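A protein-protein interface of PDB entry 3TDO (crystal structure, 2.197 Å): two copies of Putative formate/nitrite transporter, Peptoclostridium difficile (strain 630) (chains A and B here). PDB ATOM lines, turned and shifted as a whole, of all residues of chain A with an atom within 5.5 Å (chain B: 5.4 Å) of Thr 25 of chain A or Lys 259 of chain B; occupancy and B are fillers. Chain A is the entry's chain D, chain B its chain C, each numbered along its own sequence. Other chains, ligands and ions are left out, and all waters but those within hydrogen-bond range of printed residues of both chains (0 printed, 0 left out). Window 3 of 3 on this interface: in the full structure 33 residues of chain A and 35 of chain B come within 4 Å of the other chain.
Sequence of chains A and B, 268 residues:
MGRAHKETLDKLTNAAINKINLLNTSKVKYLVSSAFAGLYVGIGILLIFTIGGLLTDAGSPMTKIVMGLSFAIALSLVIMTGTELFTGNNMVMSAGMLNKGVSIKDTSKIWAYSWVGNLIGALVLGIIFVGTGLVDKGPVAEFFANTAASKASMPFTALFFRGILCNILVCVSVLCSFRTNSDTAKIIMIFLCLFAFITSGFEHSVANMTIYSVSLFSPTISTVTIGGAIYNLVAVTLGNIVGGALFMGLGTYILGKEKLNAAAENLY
The backbone carbonyl oxygen of Lys 257 of chain B is in hydrogen-bond range of the side-chain amino group of Lys 29 of chain A (2.6 Å). The backbone NH of Lys 27 of chain A lies within hydrogen-bond range of the backbone carbonyl oxygen of Tyr 268 of chain B (2.9 Å). The side-chain amino group (NZ) of Lys 259 of chain B lies within hydrogen-bond range of the backbone carbonyl oxygen (O) of Thr 25 of chain A (2.7 Å).
The backbone NH of Lys 29 of chain A is in hydrogen-bond range of the side-chain hydroxyl of Ser 26 of chain A, 3.1 Å away. The backbone carbonyl oxygen (O) of Leu 23 of chain A is in hydrogen-bond range of the side-chain amino group (NZ) of Lys 27 of chain A, at 3.4 Å. O of Asn 21 of chain A lies within hydrogen-bond range of OG1 of Thr 25 of chain A (2.8 Å).
Among the printed residues, merely in contact across the chains: Ser 26 of chain A with Leu 267 of chain B (3.98 Å), Ser 26 of chain A with Tyr 268 of chain B (3.8 Å) and Lys 29 of chain A with Leu 267 of chain B (3.8 Å).
Thr 25 of chain A touches just one residue of chain B: Lys 259. Printed residues of chain A within 4 Å of Lys 257 of chain B: Lys 29 (2.6 Å). Printed residues of chain A within 4 Å of Tyr 268 of chain B: Ser 26 and Lys 27. Printed residues of chain A within 4 Å of Leu 267 of chain B: Ser 26 and Lys 29. Asn 21 of chain A touches none of the printed residues of chain B. Asn 261 of chain B touches none of the printed residues of chain A.
Of the 9 printed residues of chain A, 4 touch a printed residue of chain B. Printed residues of chain A that touch a printed residue of chain B: Thr 25, Ser 26, Lys 27 and Lys 29. Of the 9 printed residues of chain B, 4 touch a printed residue of chain A. Among the printed residues, 6 pairs touch across the chains. Among the printed residues, no Asp or Glu carboxylate lies within 4 Å of a Lys or Arg side-chain nitrogen of the other chain.
No position is printed for both chains. Of the 6 pairs that touch across the chains among the printed residues, none has its exchanged pair printed and touching as well.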
ATOM      1  N   ILE A  20     -12.984   8.400  15.148  1.00  0.00           N
ATOM      2  CA  ILE A  20     -13.583   9.601  14.582  1.00  0.00           C
ATOM      3  C   ILE A  20     -12.887  10.863  15.096  1.00  0.00           C
ATOM      4  O   ILE A  20     -12.674  11.802  14.337  1.00  0.00           O
ATOM      5  CB  ILE A  20     -15.100   9.666  14.808  1.00  0.00           C
ATOM      6  CG1 ILE A  20     -15.667  10.947  14.186  1.00  0.00           C
ATOM      7  CG2 ILE A  20     -15.435   9.560  16.291  1.00  0.00           C
ATOM      8  CD1 ILE A  20     -15.568  10.973  12.666  1.00  0.00           C
ATOM      9  N   ASN A  21     -12.520  10.882  16.376  1.00  0.00           N
ATOM     10  CA  ASN A  21     -11.720  11.986  16.893  1.00  0.00           C
ATOM     11  C   ASN A  21     -10.429  12.131  16.094  1.00  0.00           C
ATOM     12  O   ASN A  21     -10.002  13.241  15.810  1.00  0.00           O
ATOM     13  CB  ASN A  21     -11.386  11.814  18.382  1.00  0.00           C
ATOM     14  CG  ASN A  21     -12.616  11.857  19.272  1.00  0.00           C
ATOM     15  OD1 ASN A  21     -13.670  12.360  18.883  1.00  0.00           O
ATOM     16  ND2 ASN A  21     -12.482  11.327  20.480  1.00  0.00           N
ATOM     17  N   LEU A  22      -9.807  11.011  15.725  1.00  0.00           N
ATOM     18  CA  LEU A  22      -8.587  11.083  14.926  1.00  0.00           C
ATOM     19  C   LEU A  22      -8.907  11.727  13.580  1.00  0.00           C
ATOM     20  O   LEU A  22      -8.243  12.675  13.169  1.00  0.00           O
ATOM     21  CB  LEU A  22      -7.943   9.707  14.749  1.00  0.00           C
ATOM     22  CG  LEU A  22      -6.817   9.543  13.714  1.00  0.00           C
ATOM     23  CD1 LEU A  22      -5.636  10.482  13.949  1.00  0.00           C
ATOM     24  CD2 LEU A  22      -6.325   8.085  13.669  1.00  0.00           C
ATOM     25  N   LEU A  23      -9.942  11.222  12.912  1.00  0.00           N
ATOM     26  CA  LEU A  23     -10.368  11.765  11.630  1.00  0.00           C
ATOM     27  C   LEU A  23     -10.655  13.264  11.689  1.00  0.00           C
ATOM     28  O   LEU A  23     -10.205  14.021  10.831  1.00  0.00           O
ATOM     29  CB  LEU A  23     -11.613  11.039  11.131  1.00  0.00           C
ATOM     30  CG  LEU A  23     -12.139  11.598   9.807  1.00  0.00           C
ATOM     31  CD1 LEU A  23     -11.049  11.479   8.750  1.00  0.00           C
ATOM     32  CD2 LEU A  23     -13.417  10.881   9.369  1.00  0.00           C
ATOM     33  N   ASN A  24     -11.422  13.688  12.688  1.00  0.00           N
ATOM     34  CA  ASN A  24     -11.778  15.093  12.846  1.00  0.00           C
ATOM     35  C   ASN A  24     -10.557  15.939  13.162  1.00  0.00           C
ATOM     36  O   ASN A  24     -10.448  17.086  12.740  1.00  0.00           O
ATOM     37  CB  ASN A  24     -12.772  15.262  13.991  1.00  0.00           C
ATOM     38  CG  ASN A  24     -14.142  14.767  13.646  1.00  0.00           C
ATOM     39  OD1 ASN A  24     -14.485  14.618  12.470  1.00  0.00           O
ATOM     40  ND2 ASN A  24     -14.955  14.531  14.672  1.00  0.00           N
ATOM     41  N   THR A  25      -9.650  15.364  13.940  1.00  0.00           N
ATOM     42  CA  THR A  25      -8.421  16.045  14.314  1.00  0.00           C
ATOM     43  C   THR A  25      -7.490  16.180  13.110  1.00  0.00           C
ATOM     44  O   THR A  25      -6.982  17.271  12.835  1.00  0.00           O
ATOM     45  CB  THR A  25      -7.701  15.293  15.449  1.00  0.00           C
ATOM     46  OG1 THR A  25      -8.456  15.428  16.659  1.00  0.00           O
ATOM     47  CG2 THR A  25      -6.297  15.844  15.659  1.00  0.00           C
ATOM     48  N   SER A  26      -7.246  15.066  12.420  1.00  0.00           N
ATOM     49  CA  SER A  26      -6.409  15.080  11.221  1.00  0.00           C
ATOM     50  C   SER A  26      -6.892  14.151  10.095  1.00  0.00           C
ATOM     51  O   SER A  26      -6.970  12.927  10.268  1.00  0.00           O
ATOM     52  CB  SER A  26      -4.964  14.732  11.584  1.00  0.00           C
ATOM     53  OG  SER A  26      -4.132  14.828  10.442  1.00  0.00           O
ATOM     54  N   LYS A  27      -7.159  14.725   8.927  1.00  0.00           N
ATOM     55  CA  LYS A  27      -7.523  13.923   7.768  1.00  0.00           C
ATOM     56  C   LYS A  27      -6.286  13.274   7.160  1.00  0.00           C
ATOM     57  O   LYS A  27      -6.348  12.140   6.708  1.00  0.00           O
ATOM     58  CB  LYS A  27      -8.305  14.752   6.737  1.00  0.00           C
ATOM     59  CG  LYS A  27      -9.818  14.723   6.970  1.00  0.00           C
ATOM     60  CD  LYS A  27     -10.504  16.017   6.547  1.00  0.00           C
ATOM     61  CE  LYS A  27     -11.914  16.113   7.139  1.00  0.00           C
ATOM     62  NZ  LYS A  27     -11.931  15.932   8.631  1.00  0.00           N
ATOM     63  N   LYS A  29      -3.381  12.347   8.823  1.00  0.00           N
ATOM     64  CA  LYS A  29      -3.061  11.195   9.686  1.00  0.00           C
ATOM     65  C   LYS A  29      -4.054  10.027   9.516  1.00  0.00           C
ATOM     66  O   LYS A  29      -3.657   8.850   9.546  1.00  0.00           O
ATOM     67  CB  LYS A  29      -2.980  11.589  11.169  1.00  0.00           C
ATOM     68  CG  LYS A  29      -1.844  12.539  11.534  1.00  0.00           C
ATOM     69  CD  LYS A  29      -1.983  12.967  12.984  1.00  0.00           C
ATOM     70  CE  LYS A  29      -0.670  13.434  13.580  1.00  0.00           C
ATOM     71  NZ  LYS A  29      -0.432  12.724  14.868  1.00  0.00           N
ATOM     72  N   LYS B 257       3.450  12.148  15.072  1.00  0.00           N
ATOM     73  CA  LYS B 257       3.779  13.517  15.449  1.00  0.00           C
ATOM     74  C   LYS B 257       2.545  14.223  16.002  1.00  0.00           C
ATOM     75  O   LYS B 257       1.516  14.313  15.335  1.00  0.00           O
ATOM     76  CB  LYS B 257       4.349  14.293  14.262  1.00  0.00           C
ATOM     77  CG  LYS B 257       4.865  15.680  14.629  1.00  0.00           C
ATOM     78  CD  LYS B 257       6.287  15.637  15.157  1.00  0.00           C
ATOM     79  CE  LYS B 257       6.766  17.042  15.554  1.00  0.00           C
ATOM     80  NZ  LYS B 257       8.194  17.056  15.962  1.00  0.00           N
ATOM     81  N   GLU B 258       2.649  14.718  17.229  1.00  0.00           N
ATOM     82  CA  GLU B 258       1.546  15.435  17.857  1.00  0.00           C
ATOM     83  C   GLU B 258       1.110  16.633  17.013  1.00  0.00           C
ATOM     84  O   GLU B 258       1.947  17.441  16.602  1.00  0.00           O
ATOM     85  CB  GLU B 258       1.948  15.913  19.254  1.00  0.00           C
ATOM     86  CG  GLU B 258       1.991  14.814  20.303  1.00  0.00           C
ATOM     87  CD  GLU B 258       0.996  15.045  21.427  1.00  0.00           C
ATOM     88  OE1 GLU B 258      -0.114  15.545  21.145  1.00  0.00           O
ATOM     89  OE2 GLU B 258       1.325  14.735  22.593  1.00  0.00           O
ATOM     90  N   LYS B 259      -0.196  16.744  16.766  1.00  0.00           N
ATOM     91  CA  LYS B 259      -0.742  17.843  15.971  1.00  0.00           C
ATOM     92  C   LYS B 259      -0.178  19.187  16.446  1.00  0.00           C
ATOM     93  O   LYS B 259       0.285  19.990  15.635  1.00  0.00           O
ATOM     94  CB  LYS B 259      -2.276  17.850  16.009  1.00  0.00           C
ATOM     95  CG  LYS B 259      -2.917  18.938  15.150  1.00  0.00           C
ATOM     96  CD  LYS B 259      -4.432  18.953  15.297  1.00  0.00           C
ATOM     97  CE  LYS B 259      -5.093  19.776  14.195  1.00  0.00           C
ATOM     98  NZ  LYS B 259      -6.573  19.585  14.163  1.00  0.00           N
ATOM     99  N   LEU B 260      -0.223  19.427  17.757  1.00  0.00           N
ATOM    100  CA  LEU B 260       0.516  20.542  18.342  1.00  0.00           C
ATOM    101  C   LEU B 260       1.983  20.316  18.005  1.00  0.00           C
ATOM    102  O   LEU B 260       2.471  19.193  18.070  1.00  0.00           O
ATOM    103  CB  LEU B 260       0.315  20.621  19.858  1.00  0.00           C
ATOM    104  CG  LEU B 260      -0.557  21.782  20.351  1.00  0.00           C
ATOM    105  CD1 LEU B 260      -2.035  21.453  20.197  1.00  0.00           C
ATOM    106  CD2 LEU B 260      -0.230  22.150  21.798  1.00  0.00           C
ATOM    107  N   ASN B 261       2.695  21.392  17.692  1.00  0.00           N
ATOM    108  CA  ASN B 261       3.927  21.293  16.918  1.00  0.00           C
ATOM    109  C   ASN B 261       3.666  20.737  15.514  1.00  0.00           C
ATOM    110  O   ASN B 261       3.946  19.559  15.233  1.00  0.00           O
ATOM    111  CB  ASN B 261       5.010  20.472  17.633  1.00  0.00           C
ATOM    112  CG  ASN B 261       6.410  20.700  17.048  1.00  0.00           C
ATOM    113  OD1 ASN B 261       6.568  21.273  15.969  1.00  0.00           O
ATOM    114  ND2 ASN B 261       7.428  20.240  17.767  1.00  0.00           N
ATOM    115  N   ALA B 262       3.091  21.565  14.639  1.00  0.00           N
ATOM    116  CA  ALA B 262       2.445  22.844  14.989  1.00  0.00           C
ATOM    117  C   ALA B 262       3.354  23.895  15.656  1.00  0.00           C
ATOM    118  O   ALA B 262       2.995  25.072  15.741  1.00  0.00           O
ATOM    119  CB  ALA B 262       1.177  22.620  15.816  1.00  0.00           C
ATOM    120  N   GLU B 265       4.921  23.084  11.719  1.00  0.00           N
ATOM    121  CA  GLU B 265       3.968  22.853  10.611  1.00  0.00           C
ATOM    122  C   GLU B 265       2.562  22.341  11.018  1.00  0.00           C
ATOM    123  O   GLU B 265       2.403  21.679  12.045  1.00  0.00           O
ATOM    124  CB  GLU B 265       4.577  21.863   9.614  1.00  0.00           C
ATOM    125  CG  GLU B 265       3.804  20.550   9.503  1.00  0.00           C
ATOM    126  CD  GLU B 265       4.707  19.330   9.435  1.00  0.00           C
ATOM    127  OE1 GLU B 265       5.706  19.365   8.685  1.00  0.00           O
ATOM    128  OE2 GLU B 265       4.414  18.336  10.136  1.00  0.00           O
ATOM    129  N   LEU B 267      -1.310  20.399  10.274  1.00  0.00           N
ATOM    130  CA  LEU B 267      -1.891  19.211   9.629  1.00  0.00           C
ATOM    131  C   LEU B 267      -3.378  19.325   9.267  1.00  0.00           C
ATOM    132  O   LEU B 267      -4.205  19.701  10.098  1.00  0.00           O
ATOM    133  CB  LEU B 267      -1.705  17.979  10.525  1.00  0.00           C
ATOM    134  CG  LEU B 267      -0.322  17.339  10.666  1.00  0.00           C
ATOM    135  CD1 LEU B 267      -0.078  16.861  12.092  1.00  0.00           C
ATOM    136  CD2 LEU B 267      -0.153  16.197   9.677  1.00  0.00           C
ATOM    137  N   TYR B 268      -3.713  18.966   8.031  1.00  0.00           N
ATOM    138  CA  TYR B 268      -5.104  18.909   7.589  1.00  0.00           C
ATOM    139  C   TYR B 268      -5.764  17.622   8.081  1.00  0.00           C
ATOM    140  O   TYR B 268      -6.944  17.608   8.430  1.00  0.00           O
ATOM    141  CB  TYR B 268      -5.181  18.980   6.061  1.00  0.00           C
ATOM    142  CG  TYR B 268      -6.589  19.046   5.496  1.00  0.00           C
ATOM    143  CD1 TYR B 268      -7.691  19.224   6.327  1.00  0.00           C
ATOM    144  CD2 TYR B 268      -6.813  18.923   4.128  1.00  0.00           C
ATOM    145  CE1 TYR B 268      -8.975  19.285   5.811  1.00  0.00           C
ATOM    146  CE2 TYR B 268      -8.092  18.981   3.604  1.00  0.00           C
ATOM    147  CZ  TYR B 268      -9.170  19.162   4.450  1.00  0.00           C
ATOM    148  OH  TYR B 268     -10.446  19.220   3.931  1.00  0.00           O
